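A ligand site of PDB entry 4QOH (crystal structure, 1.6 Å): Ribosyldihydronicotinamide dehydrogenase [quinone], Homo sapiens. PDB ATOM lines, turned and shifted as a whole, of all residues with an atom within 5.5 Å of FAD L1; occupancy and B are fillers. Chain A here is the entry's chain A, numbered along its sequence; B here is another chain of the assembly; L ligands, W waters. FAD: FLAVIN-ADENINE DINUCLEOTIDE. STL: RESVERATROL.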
ATOM      1  N   HIS A  12       1.338 -21.503 -31.618  1.00  0.00           N
ATOM      2  CA  HIS A  12       1.338 -20.484 -30.550  1.00  0.00           C
ATOM      3  C   HIS A  12       0.289 -19.431 -30.925  1.00  0.00           C
ATOM      4  O   HIS A  12       0.205 -19.029 -32.089  1.00  0.00           O
ATOM      5  CB  HIS A  12       2.652 -19.877 -30.346  1.00  0.00           C
ATOM      6  CG  HIS A  12       2.769 -19.212 -28.987  1.00  0.00           C
ATOM      7  ND1 HIS A  12       2.074 -18.054 -28.669  1.00  0.00           N
ATOM      8  CD2 HIS A  12       3.518 -19.506 -27.908  1.00  0.00           C
ATOM      9  CE1 HIS A  12       2.331 -17.722 -27.425  1.00  0.00           C
ATOM     10  NE2 HIS A  12       3.257 -18.521 -26.955  1.00  0.00           N
ATOM     11  N   LYS A  16       3.482 -12.025 -31.308  1.00  0.00           N
ATOM     12  CA  LYS A  16       4.596 -11.346 -30.601  1.00  0.00           C
ATOM     13  C   LYS A  16       5.318 -12.220 -29.563  1.00  0.00           C
ATOM     14  O   LYS A  16       6.242 -11.786 -28.898  1.00  0.00           O
ATOM     15  CB  LYS A  16       4.109 -10.034 -29.928  1.00  0.00           C
ATOM     16  CG  LYS A  16       3.509  -9.073 -30.916  1.00  0.00           C
ATOM     17  CD  LYS A  16       2.935  -7.868 -30.206  1.00  0.00           C
ATOM     18  CE  LYS A  16       2.701  -6.671 -31.145  1.00  0.00           C
ATOM     19  NZ  LYS A  16       1.278  -6.620 -31.594  1.00  0.00           N
ATOM     20  N   SER A  17       4.859 -13.452 -29.405  1.00  0.00           N
ATOM     21  CA  SER A  17       5.476 -14.364 -28.445  1.00  0.00           C
ATOM     22  C   SER A  17       6.903 -14.744 -28.778  1.00  0.00           C
ATOM     23  O   SER A  17       7.381 -14.504 -29.875  1.00  0.00           O
ATOM     24  CB  SER A  17       4.573 -15.621 -28.343  1.00  0.00           C
ATOM     25  OG  SER A  17       4.781 -16.481 -29.504  1.00  0.00           O
ATOM     26  N   PHE A  18       7.584 -15.355 -27.842  1.00  0.00           N
ATOM     27  CA  PHE A  18       8.917 -15.890 -28.089  1.00  0.00           C
ATOM     28  C   PHE A  18       8.870 -17.020 -29.146  1.00  0.00           C
ATOM     29  O   PHE A  18       9.745 -17.042 -30.014  1.00  0.00           O
ATOM     30  CB  PHE A  18       9.497 -16.460 -26.814  1.00  0.00           C
ATOM     31  CG  PHE A  18      10.956 -16.718 -26.853  1.00  0.00           C
ATOM     32  CD1 PHE A  18      11.864 -15.665 -26.776  1.00  0.00           C
ATOM     33  CD2 PHE A  18      11.446 -17.996 -26.955  1.00  0.00           C
ATOM     34  CE1 PHE A  18      13.200 -15.878 -26.815  1.00  0.00           C
ATOM     35  CE2 PHE A  18      12.793 -18.238 -27.003  1.00  0.00           C
ATOM     36  CZ  PHE A  18      13.681 -17.183 -26.913  1.00  0.00           C
ATOM     37  N   ASN A  19       7.859 -17.891 -29.071  1.00  0.00           N
ATOM     38  CA  ASN A  19       7.602 -18.840 -30.188  1.00  0.00           C
ATOM     39  C   ASN A  19       7.432 -18.125 -31.516  1.00  0.00           C
ATOM     40  O   ASN A  19       8.012 -18.512 -32.496  1.00  0.00           O
ATOM     41  CB  ASN A  19       6.426 -19.778 -29.903  1.00  0.00           C
ATOM     42  CG  ASN A  19       6.851 -20.953 -29.081  1.00  0.00           C
ATOM     43  OD1 ASN A  19       7.107 -22.054 -29.657  1.00  0.00           O
ATOM     44  ND2 ASN A  19       6.969 -20.801 -27.801  1.00  0.00           N
ATOM     45  N   GLY A  20       6.644 -17.052 -31.574  1.00  0.00           N
ATOM     46  CA  GLY A  20       6.492 -16.335 -32.816  1.00  0.00           C
ATOM     47  C   GLY A  20       7.787 -15.796 -33.356  1.00  0.00           C
ATOM     48  O   GLY A  20       8.030 -15.797 -34.556  1.00  0.00           O
ATOM     49  N   SER A  21       8.685 -15.341 -32.474  1.00  0.00           N
ATOM     50  CA  SER A  21       9.974 -14.782 -32.923  1.00  0.00           C
ATOM     51  C   SER A  21      10.916 -15.871 -33.484  1.00  0.00           C
ATOM     52  O   SER A  21      11.737 -15.625 -34.376  1.00  0.00           O
ATOM     53  CB  SER A  21      10.673 -14.130 -31.717  1.00  0.00           C
ATOM     54  OG  SER A  21       9.914 -13.026 -31.283  1.00  0.00           O
ATOM     55  N   PRO A 103       5.534 -24.167 -27.696  1.00  0.00           N
ATOM     56  CA  PRO A 103       5.801 -24.213 -26.289  1.00  0.00           C
ATOM     57  C   PRO A 103       5.503 -25.655 -25.762  1.00  0.00           C
ATOM     58  O   PRO A 103       4.481 -26.206 -26.152  1.00  0.00           O
ATOM     59  CB  PRO A 103       4.819 -23.186 -25.726  1.00  0.00           C
ATOM     60  CG  PRO A 103       3.647 -23.256 -26.682  1.00  0.00           C
ATOM     61  CD  PRO A 103       4.262 -23.508 -28.004  1.00  0.00           C
ATOM     62  N   LEU A 104       6.364 -26.194 -24.908  1.00  0.00           N
ATOM     63  CA  LEU A 104       6.022 -27.370 -24.160  1.00  0.00           C
ATOM     64  C   LEU A 104       4.781 -27.195 -23.309  1.00  0.00           C
ATOM     65  O   LEU A 104       4.698 -26.282 -22.468  1.00  0.00           O
ATOM     66  CB  LEU A 104       7.201 -27.818 -23.295  1.00  0.00           C
ATOM     67  CG  LEU A 104       7.336 -29.246 -22.868  1.00  0.00           C
ATOM     68  CD1 LEU A 104       7.533 -30.172 -24.076  1.00  0.00           C
ATOM     69  CD2 LEU A 104       8.420 -29.302 -21.748  1.00  0.00           C
ATOM     70  N   TYR A 105       3.774 -27.962 -23.520  1.00  0.00           N
ATOM     71  CA  TYR A 105       2.587 -28.157 -22.663  1.00  0.00           C
ATOM     72  C   TYR A 105       2.544 -29.519 -22.069  1.00  0.00           C
ATOM     73  O   TYR A 105       2.452 -30.531 -22.882  1.00  0.00           O
ATOM     74  CB  TYR A 105       1.322 -27.974 -23.513  1.00  0.00           C
ATOM     75  CG  TYR A 105       0.862 -26.564 -23.857  1.00  0.00           C
ATOM     76  CD1 TYR A 105       1.721 -25.468 -23.765  1.00  0.00           C
ATOM     77  CD2 TYR A 105      -0.430 -26.337 -24.295  1.00  0.00           C
ATOM     78  CE1 TYR A 105       1.262 -24.195 -24.105  1.00  0.00           C
ATOM     79  CE2 TYR A 105      -0.898 -25.050 -24.577  1.00  0.00           C
ATOM     80  CZ  TYR A 105      -0.014 -24.000 -24.521  1.00  0.00           C
ATOM     81  OH  TYR A 105      -0.532 -22.758 -24.857  1.00  0.00           O
ATOM     82  N   TRP A 106       2.686 -29.687 -20.777  1.00  0.00           N
ATOM     83  CA  TRP A 106       2.641 -30.970 -20.095  1.00  0.00           C
ATOM     84  C   TRP A 106       3.605 -32.033 -20.680  1.00  0.00           C
ATOM     85  O   TRP A 106       3.142 -33.115 -21.097  1.00  0.00           O
ATOM     86  CB  TRP A 106       1.183 -31.524 -20.059  1.00  0.00           C
ATOM     87  CG  TRP A 106       0.206 -30.572 -19.326  1.00  0.00           C
ATOM     88  CD1 TRP A 106      -0.949 -30.065 -19.757  1.00  0.00           C
ATOM     89  CD2 TRP A 106       0.411 -30.096 -18.024  1.00  0.00           C
ATOM     90  NE1 TRP A 106      -1.469 -29.187 -18.819  1.00  0.00           N
ATOM     91  CE2 TRP A 106      -0.698 -29.275 -17.698  1.00  0.00           C
ATOM     92  CE3 TRP A 106       1.394 -30.358 -17.050  1.00  0.00           C
ATOM     93  CZ2 TRP A 106      -0.795 -28.641 -16.472  1.00  0.00           C
ATOM     94  CZ3 TRP A 106       1.309 -29.705 -15.816  1.00  0.00           C
ATOM     95  CH2 TRP A 106       0.222 -28.878 -15.540  1.00  0.00           C
ATOM     96  N   PHE A 107       4.856 -31.643 -20.851  1.00  0.00           N
ATOM     97  CA  PHE A 107       5.929 -32.470 -21.349  1.00  0.00           C
ATOM     98  C   PHE A 107       5.669 -32.954 -22.756  1.00  0.00           C
ATOM     99  O   PHE A 107       6.180 -33.947 -23.123  1.00  0.00           O
ATOM    100  CB  PHE A 107       6.209 -33.649 -20.435  1.00  0.00           C
ATOM    101  CG  PHE A 107       7.055 -33.362 -19.216  1.00  0.00           C
ATOM    102  CD1 PHE A 107       7.102 -32.137 -18.649  1.00  0.00           C
ATOM    103  CD2 PHE A 107       7.778 -34.377 -18.626  1.00  0.00           C
ATOM    104  CE1 PHE A 107       7.848 -31.912 -17.504  1.00  0.00           C
ATOM    105  CE2 PHE A 107       8.537 -34.161 -17.504  1.00  0.00           C
ATOM    106  CZ  PHE A 107       8.560 -32.919 -16.932  1.00  0.00           C
ATOM    107  N   SER A 108       4.900 -32.202 -23.523  1.00  0.00           N
ATOM    108  CA  SER A 108       4.470 -32.636 -24.839  1.00  0.00           C
ATOM    109  C   SER A 108       4.094 -31.452 -25.714  1.00  0.00           C
ATOM    110  O   SER A 108       4.385 -30.374 -25.407  1.00  0.00           O
ATOM    111  CB  SER A 108       3.315 -33.564 -24.657  1.00  0.00           C
ATOM    112  OG  SER A 108       2.934 -34.198 -25.840  1.00  0.00           O
ATOM    113  N   THR A 148      10.102 -24.555 -26.688  1.00  0.00           N
ATOM    114  CA  THR A 148      10.329 -23.612 -25.585  1.00  0.00           C
ATOM    115  C   THR A 148       9.739 -24.136 -24.309  1.00  0.00           C
ATOM    116  O   THR A 148       8.768 -24.866 -24.300  1.00  0.00           O
ATOM    117  CB  THR A 148       9.725 -22.217 -25.882  1.00  0.00           C
ATOM    118  OG1 THR A 148       8.323 -22.237 -25.865  1.00  0.00           O
ATOM    119  CG2 THR A 148      10.225 -21.655 -27.249  1.00  0.00           C
ATOM    120  N   THR A 149      10.311 -23.759 -23.140  1.00  0.00           N
ATOM    121  CA  THR A 149       9.869 -24.366 -21.895  1.00  0.00           C
ATOM    122  C   THR A 149       9.625 -23.312 -20.831  1.00  0.00           C
ATOM    123  O   THR A 149      10.223 -22.278 -20.884  1.00  0.00           O
ATOM    124  CB  THR A 149      10.856 -25.430 -21.337  1.00  0.00           C
ATOM    125  OG1 THR A 149      12.086 -24.800 -20.862  1.00  0.00           O
ATOM    126  CG2 THR A 149      11.153 -26.581 -22.332  1.00  0.00           C
ATOM    127  N   GLY A 150       8.807 -23.632 -19.840  1.00  0.00           N
ATOM    128  CA  GLY A 150       8.711 -22.821 -18.606  1.00  0.00           C
ATOM    129  C   GLY A 150       9.867 -23.144 -17.658  1.00  0.00           C
ATOM    130  O   GLY A 150      10.445 -22.264 -17.044  1.00  0.00           O
ATOM    131  N   GLY A 151      10.197 -24.440 -17.559  1.00  0.00           N
ATOM    132  CA  GLY A 151      11.237 -24.978 -16.718  1.00  0.00           C
ATOM    133  C   GLY A 151      12.651 -24.697 -17.218  1.00  0.00           C
ATOM    134  O   GLY A 151      12.883 -24.578 -18.412  1.00  0.00           O
ATOM    135  N   TYR A 156      15.485 -29.399 -16.032  1.00  0.00           N
ATOM    136  CA  TYR A 156      15.554 -30.453 -16.996  1.00  0.00           C
ATOM    137  C   TYR A 156      16.898 -31.152 -17.078  1.00  0.00           C
ATOM    138  O   TYR A 156      17.397 -31.388 -18.102  1.00  0.00           O
ATOM    139  CB  TYR A 156      15.076 -30.028 -18.388  1.00  0.00           C
ATOM    140  CG  TYR A 156      13.609 -29.755 -18.445  1.00  0.00           C
ATOM    141  CD1 TYR A 156      12.696 -30.779 -18.579  1.00  0.00           C
ATOM    142  CD2 TYR A 156      13.142 -28.481 -18.397  1.00  0.00           C
ATOM    143  CE1 TYR A 156      11.372 -30.499 -18.645  1.00  0.00           C
ATOM    144  CE2 TYR A 156      11.826 -28.211 -18.463  1.00  0.00           C
ATOM    145  CZ  TYR A 156      10.957 -29.225 -18.585  1.00  0.00           C
ATOM    146  OH  TYR A 156       9.663 -28.935 -18.621  1.00  0.00           O
ATOM    147  N   ASN A 162      12.415 -32.048 -13.070  1.00  0.00           N
ATOM    148  CA  ASN A 162      11.754 -32.479 -14.327  1.00  0.00           C
ATOM    149  C   ASN A 162      12.407 -33.655 -15.056  1.00  0.00           C
ATOM    150  O   ASN A 162      11.863 -34.266 -16.073  1.00  0.00           O
ATOM    151  CB  ASN A 162      11.645 -31.246 -15.202  1.00  0.00           C
ATOM    152  CG  ASN A 162      10.731 -30.208 -14.648  1.00  0.00           C
ATOM    153  OD1 ASN A 162       9.975 -30.395 -13.684  1.00  0.00           O
ATOM    154  ND2 ASN A 162      10.733 -29.089 -15.306  1.00  0.00           N
ATOM    155  N   PRO A 193      12.377 -18.873 -21.521  1.00  0.00           N
ATOM    156  CA  PRO A 193      12.535 -17.475 -21.903  1.00  0.00           C
ATOM    157  C   PRO A 193      11.945 -16.513 -20.901  1.00  0.00           C
ATOM    158  O   PRO A 193      12.494 -15.413 -20.742  1.00  0.00           O
ATOM    159  CB  PRO A 193      11.779 -17.380 -23.233  1.00  0.00           C
ATOM    160  CG  PRO A 193      10.816 -18.526 -23.183  1.00  0.00           C
ATOM    161  CD  PRO A 193      11.613 -19.641 -22.538  1.00  0.00           C
ATOM    162  N   GLU A 194      10.843 -16.864 -20.251  1.00  0.00           N
ATOM    163  CA  GLU A 194      10.130 -15.885 -19.392  1.00  0.00           C
ATOM    164  C   GLU A 194      11.072 -15.428 -18.221  1.00  0.00           C
ATOM    165  O   GLU A 194      10.990 -14.318 -17.740  1.00  0.00           O
ATOM    166  CB  GLU A 194       8.780 -16.514 -18.949  1.00  0.00           C
ATOM    167  CG  GLU A 194       7.813 -16.671 -20.158  1.00  0.00           C
ATOM    168  CD  GLU A 194       6.582 -17.609 -20.014  1.00  0.00           C
ATOM    169  OE1 GLU A 194       6.677 -18.873 -19.803  1.00  0.00           O
ATOM    170  OE2 GLU A 194       5.473 -17.038 -20.231  1.00  0.00           O
ATOM    171  N   GLU A 198      16.038  -9.837 -21.257  1.00  0.00           N
ATOM    172  CA  GLU A 198      15.910  -9.453 -22.678  1.00  0.00           C
ATOM    173  C   GLU A 198      17.090  -9.903 -23.557  1.00  0.00           C
ATOM    174  O   GLU A 198      16.909 -10.311 -24.702  1.00  0.00           O
ATOM    175  CB  GLU A 198      15.726  -7.930 -22.863  1.00  0.00           C
ATOM    176  CG  GLU A 198      14.280  -7.513 -23.085  1.00  0.00           C
ATOM    177  CD  GLU A 198      13.659  -8.139 -24.327  1.00  0.00           C
ATOM    178  OE1 GLU A 198      14.222  -7.929 -25.416  1.00  0.00           O
ATOM    179  OE2 GLU A 198      12.618  -8.847 -24.221  1.00  0.00           O
ATOM    180  N   ARG A 201      17.273 -13.688 -23.982  1.00  0.00           N
ATOM    181  CA  ARG A 201      16.246 -14.030 -24.997  1.00  0.00           C
ATOM    182  C   ARG A 201      16.720 -13.796 -26.410  1.00  0.00           C
ATOM    183  O   ARG A 201      16.658 -14.702 -27.249  1.00  0.00           O
ATOM    184  CB  ARG A 201      14.993 -13.268 -24.735  1.00  0.00           C
ATOM    185  CG  ARG A 201      14.378 -13.748 -23.440  1.00  0.00           C
ATOM    186  CD  ARG A 201      12.933 -13.471 -23.435  1.00  0.00           C
ATOM    187  NE  ARG A 201      12.681 -12.102 -23.048  1.00  0.00           N
ATOM    188  CZ  ARG A 201      12.479 -11.694 -21.799  1.00  0.00           C
ATOM    189  NH1 ARG A 201      12.193 -10.430 -21.586  1.00  0.00           N
ATOM    190  NH2 ARG A 201      12.568 -12.544 -20.770  1.00  0.00           N
ATOM    191  N   LYS A 202      17.242 -12.592 -26.676  1.00  0.00           N
ATOM    192  CA  LYS A 202      17.893 -12.267 -27.951  1.00  0.00           C
ATOM    193  C   LYS A 202      18.913 -13.290 -28.383  1.00  0.00           C
ATOM    194  O   LYS A 202      18.887 -13.772 -29.532  1.00  0.00           O
ATOM    195  CB  LYS A 202      18.550 -10.905 -27.861  1.00  0.00           C
ATOM    196  CG  LYS A 202      17.519  -9.808 -27.816  1.00  0.00           C
ATOM    197  CD  LYS A 202      17.218  -9.261 -29.192  1.00  0.00           C
ATOM    198  CE  LYS A 202      15.946  -8.395 -29.180  1.00  0.00           C
ATOM    199  NZ  LYS A 202      15.954  -7.386 -28.070  1.00  0.00           N
ATOM    200  N   VAL A 205      17.191 -16.418 -29.601  1.00  0.00           N
ATOM    201  CA  VAL A 205      16.653 -16.226 -30.968  1.00  0.00           C
ATOM    202  C   VAL A 205      17.814 -16.267 -31.986  1.00  0.00           C
ATOM    203  O   VAL A 205      17.745 -16.962 -33.015  1.00  0.00           O
ATOM    204  CB  VAL A 205      15.810 -14.934 -31.067  1.00  0.00           C
ATOM    205  CG1 VAL A 205      15.359 -14.702 -32.496  1.00  0.00           C
ATOM    206  CG2 VAL A 205      14.589 -14.989 -30.181  1.00  0.00           C
ATOM    207  N   ASN B  67      -1.205 -13.895 -23.639  1.00  0.00           N
ATOM    208  CA  ASN B  67      -0.462 -14.942 -22.940  1.00  0.00           C
ATOM    209  C   ASN B  67      -1.448 -15.962 -22.285  1.00  0.00           C
ATOM    210  O   ASN B  67      -2.123 -15.691 -21.295  1.00  0.00           O
ATOM    211  CB  ASN B  67       0.403 -14.291 -21.897  1.00  0.00           C
ATOM    212  CG  ASN B  67       1.298 -15.267 -21.219  1.00  0.00           C
ATOM    213  OD1 ASN B  67       0.905 -16.352 -20.809  1.00  0.00           O
ATOM    214  ND2 ASN B  67       2.545 -14.907 -21.116  1.00  0.00           N
ATOM    215  N   TYR B  68      -1.554 -17.144 -22.859  1.00  0.00           N
ATOM    216  CA  TYR B  68      -2.474 -18.091 -22.334  1.00  0.00           C
ATOM    217  C   TYR B  68      -2.333 -18.443 -20.884  1.00  0.00           C
ATOM    218  O   TYR B  68      -3.360 -18.497 -20.182  1.00  0.00           O
ATOM    219  CB  TYR B  68      -2.433 -19.420 -23.187  1.00  0.00           C
ATOM    220  CG  TYR B  68      -3.581 -20.358 -22.852  1.00  0.00           C
ATOM    221  CD1 TYR B  68      -4.888 -20.140 -23.363  1.00  0.00           C
ATOM    222  CD2 TYR B  68      -3.392 -21.454 -22.030  1.00  0.00           C
ATOM    223  CE1 TYR B  68      -5.972 -20.968 -23.010  1.00  0.00           C
ATOM    224  CE2 TYR B  68      -4.448 -22.287 -21.686  1.00  0.00           C
ATOM    225  CZ  TYR B  68      -5.719 -22.103 -22.189  1.00  0.00           C
ATOM    226  OH  TYR B  68      -6.815 -22.894 -21.823  1.00  0.00           O
ATOM    227  N   GLY B  69      -1.132 -18.818 -20.437  1.00  0.00           N
ATOM    228  CA  GLY B  69      -0.872 -19.289 -19.062  1.00  0.00           C
ATOM    229  C   GLY B  69      -1.283 -18.186 -18.059  1.00  0.00           C
ATOM    230  O   GLY B  69      -2.026 -18.428 -17.117  1.00  0.00           O
ATOM    231  N   ASP B 118      -4.589 -29.711 -21.007  1.00  0.00           N
ATOM    232  CA  ASP B 118      -4.018 -28.411 -21.275  1.00  0.00           C
ATOM    233  C   ASP B 118      -4.894 -27.338 -20.672  1.00  0.00           C
ATOM    234  O   ASP B 118      -4.380 -26.389 -20.139  1.00  0.00           O
ATOM    235  CB  ASP B 118      -3.903 -28.115 -22.767  1.00  0.00           C
ATOM    236  CG  ASP B 118      -2.842 -28.949 -23.491  1.00  0.00           C
ATOM    237  OD1 ASP B 118      -2.074 -29.638 -22.869  1.00  0.00           O
ATOM    238  OD2 ASP B 118      -2.805 -28.827 -24.683  1.00  0.00           O
ATOM    239  N   GLY B 175       5.148 -35.380 -15.620  1.00  0.00           N
ATOM    240  CA  GLY B 175       5.109 -34.042 -16.096  1.00  0.00           C
ATOM    241  C   GLY B 175       3.730 -33.381 -15.882  1.00  0.00           C
ATOM    242  O   GLY B 175       3.586 -32.172 -15.757  1.00  0.00           O
HETATM  243  PA  FAD L   1       6.615 -15.638 -24.150  1.00  0.00           P
HETATM  244  O1A FAD L   1       5.910 -15.605 -22.903  1.00  0.00           O
HETATM  245  O2A FAD L   1       5.911 -15.123 -25.386  1.00  0.00           O
HETATM  246  O5B FAD L   1       8.064 -15.082 -24.192  1.00  0.00           O
HETATM  247  C5B FAD L   1       8.755 -14.742 -22.995  1.00  0.00           C
HETATM  248  C4B FAD L   1       9.234 -13.321 -23.208  1.00  0.00           C
HETATM  249  O4B FAD L   1      10.050 -13.238 -24.397  1.00  0.00           O
HETATM  250  C3B FAD L   1       8.103 -12.313 -23.379  1.00  0.00           C
HETATM  251  O3B FAD L   1       8.227 -11.197 -22.521  1.00  0.00           O
HETATM  252  C2B FAD L   1       8.275 -11.836 -24.817  1.00  0.00           C
HETATM  253  O2B FAD L   1       7.996 -10.455 -24.852  1.00  0.00           O
HETATM  254  C1B FAD L   1       9.758 -11.991 -24.986  1.00  0.00           C
HETATM  255  N9A FAD L   1      10.201 -11.975 -26.355  1.00  0.00           N
HETATM  256  C8A FAD L   1       9.465 -12.273 -27.466  1.00  0.00           C
HETATM  257  N7A FAD L   1      10.126 -12.168 -28.596  1.00  0.00           N
HETATM  258  C5A FAD L   1      11.401 -11.783 -28.188  1.00  0.00           C
HETATM  259  C6A FAD L   1      12.579 -11.512 -28.910  1.00  0.00           C
HETATM  260  N6A FAD L   1      12.690 -11.641 -30.234  1.00  0.00           N
HETATM  261  N1A FAD L   1      13.667 -11.124 -28.213  1.00  0.00           N
HETATM  262  C2A FAD L   1      13.569 -11.029 -26.884  1.00  0.00           C
HETATM  263  N3A FAD L   1      12.520 -11.279 -26.091  1.00  0.00           N
HETATM  264  C4A FAD L   1      11.454 -11.650 -26.817  1.00  0.00           C
HETATM  265  N1  FAD L   1       6.643 -25.544 -19.142  1.00  0.00           N
HETATM  266  C2  FAD L   1       7.427 -26.625 -18.894  1.00  0.00           C
HETATM  267  O2  FAD L   1       8.657 -26.542 -18.716  1.00  0.00           O
HETATM  268  N3  FAD L   1       6.841 -27.890 -18.871  1.00  0.00           N
HETATM  269  C4  FAD L   1       5.495 -28.184 -19.098  1.00  0.00           C
HETATM  270  O4  FAD L   1       5.117 -29.359 -19.080  1.00  0.00           O
HETATM  271  C4X FAD L   1       4.683 -27.025 -19.349  1.00  0.00           C
HETATM  272  N5  FAD L   1       3.398 -27.199 -19.513  1.00  0.00           N
HETATM  273  C5X FAD L   1       2.626 -26.119 -19.779  1.00  0.00           C
HETATM  274  C6  FAD L   1       1.258 -26.290 -19.964  1.00  0.00           C
HETATM  275  C7  FAD L   1       0.445 -25.224 -20.341  1.00  0.00           C
HETATM  276  C7M FAD L   1      -1.039 -25.446 -20.536  1.00  0.00           C
HETATM  277  C8  FAD L   1       1.018 -23.963 -20.533  1.00  0.00           C
HETATM  278  C8M FAD L   1       0.157 -22.796 -20.874  1.00  0.00           C
HETATM  279  C9  FAD L   1       2.375 -23.768 -20.286  1.00  0.00           C
HETATM  280  C9A FAD L   1       3.188 -24.834 -19.909  1.00  0.00           C
HETATM  281  N10 FAD L   1       4.532 -24.688 -19.658  1.00  0.00           N
HETATM  282  C10 FAD L   1       5.336 -25.759 -19.361  1.00  0.00           C
HETATM  283  C1' FAD L   1       5.197 -23.399 -19.887  1.00  0.00           C
HETATM  284  C2' FAD L   1       5.405 -23.032 -21.347  1.00  0.00           C
HETATM  285  O2' FAD L   1       6.213 -24.037 -22.006  1.00  0.00           O
HETATM  286  C3' FAD L   1       6.112 -21.684 -21.507  1.00  0.00           C
HETATM  287  O3' FAD L   1       5.267 -20.704 -20.892  1.00  0.00           O
HETATM  288  C4' FAD L   1       6.384 -21.301 -22.963  1.00  0.00           C
HETATM  289  O4' FAD L   1       7.351 -22.251 -23.437  1.00  0.00           O
HETATM  290  C5' FAD L   1       7.018 -19.928 -23.097  1.00  0.00           C
HETATM  291  O5' FAD L   1       7.099 -19.571 -24.494  1.00  0.00           O
HETATM  292  P   FAD L   1       6.255 -18.389 -25.080  1.00  0.00           P
HETATM  293  O1P FAD L   1       6.639 -18.130 -26.494  1.00  0.00           O
HETATM  294  O2P FAD L   1       4.871 -18.439 -24.672  1.00  0.00           O
HETATM  295  O3P FAD L   1       7.040 -17.192 -24.256  1.00  0.00           O
HETATM  296  C1  STL L   2       5.924 -29.304 -15.583  1.00  0.00           C
HETATM  297  C2  STL L   2       7.190 -28.781 -15.354  1.00  0.00           C
HETATM  298  C3  STL L   2       7.376 -27.411 -15.435  1.00  0.00           C
HETATM  299  C4  STL L   2       6.332 -26.569 -15.707  1.00  0.00           C
HETATM  300  C5  STL L   2       5.053 -27.066 -15.944  1.00  0.00           C
HETATM  301  C6  STL L   2       4.854 -28.468 -15.892  1.00  0.00           C
HETATM  302  C7  STL L   2       4.083 -25.976 -16.221  1.00  0.00           C
HETATM  303  C8  STL L   2       2.840 -26.002 -16.489  1.00  0.00           C
HETATM  304  C9  STL L   2       1.852 -24.928 -16.761  1.00  0.00           C
HETATM  305  C10 STL L   2       0.625 -25.546 -16.973  1.00  0.00           C
HETATM  306  C11 STL L   2      -0.513 -24.821 -17.275  1.00  0.00           C
HETATM  307  C12 STL L   2      -0.448 -23.444 -17.392  1.00  0.00           C
HETATM  308  C13 STL L   2       0.767 -22.789 -17.167  1.00  0.00           C
HETATM  309  C14 STL L   2       1.901 -23.527 -16.862  1.00  0.00           C
HETATM  310  O1  STL L   2      -1.626 -22.903 -17.849  1.00  0.00           O
HETATM  311  O2  STL L   2       8.623 -26.895 -15.198  1.00  0.00           O
HETATM  312  O3  STL L   2       5.909 -30.685 -15.471  1.00  0.00           O
HETATM  313  O   HOH W   1       2.896 -20.390 -24.017  1.00  0.00           O
HETATM  314  O   HOH W   2      15.334 -11.022 -31.642  1.00  0.00           O
HETATM  315  O   HOH W   3       5.711 -10.922 -26.318  1.00  0.00           O
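Water W3 lies within hydrogen-bond range of an oxygen (O2B) of FAD L1 (2.8 Å) and the backbone carbonyl oxygen of Lys 16 (2.8 Å).
The side-chain carboxylate (OE2) of Glu 198 sits close to a nitrogen (N3A) of FAD L1 (3.1 Å).
Lys 16 touches FAD L1 (O to C8A, 3.6 Å).
Ser 17 touches FAD L1.
CB of Pro 103 touches O4' of FAD L1, 3.5 Å away.
CA of Tyr 105 touches N5 of FAD L1 (3.4 Å).
CE of Lys 202 touches N1A of FAD L1, 3.7 Å away.
Val 205 touches FAD L1 (CG2 to N6A, 3.8 Å).
ND2 of Asn 67 of chain B touches O1A of FAD L1, at 3.9 Å.
Tyr 68 of chain B touches FAD L1 (CD2 to C8M, 3.97 Å).
Asp 118 of chain B touches FAD L1 (O to C7M, 3.5 Å).
Hydrophobic or aromatic side chains within 4 Å of FAD L1: His 12, Phe 18, Pro 103, Leu 104, Tyr 105, Phe 107, Tyr 156, Val 205 and Tyr 68 of chain B.
The backbone NH of Gly 69 of chain B sits at hydrogen-bond distance from the side-chain amide oxygen of Asn 67 of chain B (3.2 Å).
A ring nitrogen (ND1) of His 12 is in hydrogen-bond range of the side-chain hydroxyl (OG) of Ser 17.
NH1 of Arg 201 lies within salt-bridge range of OE2 of Glu 198 (3.1 Å).
The backbone NH (N) of Asn 19 sits close to the side-chain hydroxyl (OG) of Ser 17 (3.4 Å).
The backbone carbonyl oxygen (O) of Pro 193 is in hydrogen-bond range of the guanidinium group (NH2) of Arg 201 (2.9 Å).
The side-chain hydroxyl of Tyr 156 sits close to the side-chain amide nitrogen of Asn 162 (3.5 Å).
The side-chain hydroxyl (OG) of Ser 17 sits at hydrogen-bond distance from the backbone NH (N) of Gly 20, at 2.8 Å.
OG1 of Thr 149 sits at hydrogen-bond distance from O of Gly 151 (2.6 Å).
The backbone carbonyl oxygen (O) of Thr 148 sits at hydrogen-bond distance from an oxygen (O4') of FAD L1, 3.1 Å away.
The backbone NH (N) of Gly 151 sits at hydrogen-bond distance from an oxygen (O2) of FAD L1, at 2.9 Å.
An oxygen (O2) of FAD L1 is in hydrogen-bond range of the side-chain hydroxyl of Tyr 156 (2.6 Å).
An oxygen (O4') of FAD L1 is in hydrogen-bond range of the side-chain hydroxyl of Thr 148.
The backbone NH (N) of Trp 106 lies within hydrogen-bond range of a nitrogen (N5) of FAD L1 (2.9 Å).
An oxygen (O2') of FAD L1 sits at hydrogen-bond distance from the backbone carbonyl oxygen (O) of Leu 104 (2.7 Å).
N of Asn 19 lies within hydrogen-bond range of O1P of FAD L1, 2.9 Å away.
The backbone NH (N) of Thr 149 lies within hydrogen-bond range of an oxygen (O4') of FAD L1.
The backbone NH of Gly 150 lies within hydrogen-bond range of a nitrogen (N1) of FAD L1 (3.0 Å).
O2 of STL L2 sits at hydrogen-bond distance from ND2 of Asn 162, 3.0 Å away.
O3' of FAD L1 lies within hydrogen-bond range of OE1 of Glu 194, 2.6 Å away.
The side-chain hydroxyl of Ser 21 sits at hydrogen-bond distance from a nitrogen (N7A) of FAD L1 (2.8 Å).
O2P of FAD L1 sits at hydrogen-bond distance from NE2 of His 12.
The guanidinium group of Arg 201 is in hydrogen-bond range of a nitrogen (N3A) of FAD L1, at 3.2 Å.
The backbone NH (N) of Phe 18 lies within hydrogen-bond range of an oxygen (O2A) of FAD L1 (3.0 Å).
O of Gly 175 of chain B sits at hydrogen-bond distance from O3 of STL L2 (2.8 Å).
N of Phe 107 sits at hydrogen-bond distance from O4 of FAD L1, at 2.9 Å.
The side-chain amide nitrogen (ND2) of Asn 19 is in hydrogen-bond range of an oxygen (O1P) of FAD L1.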
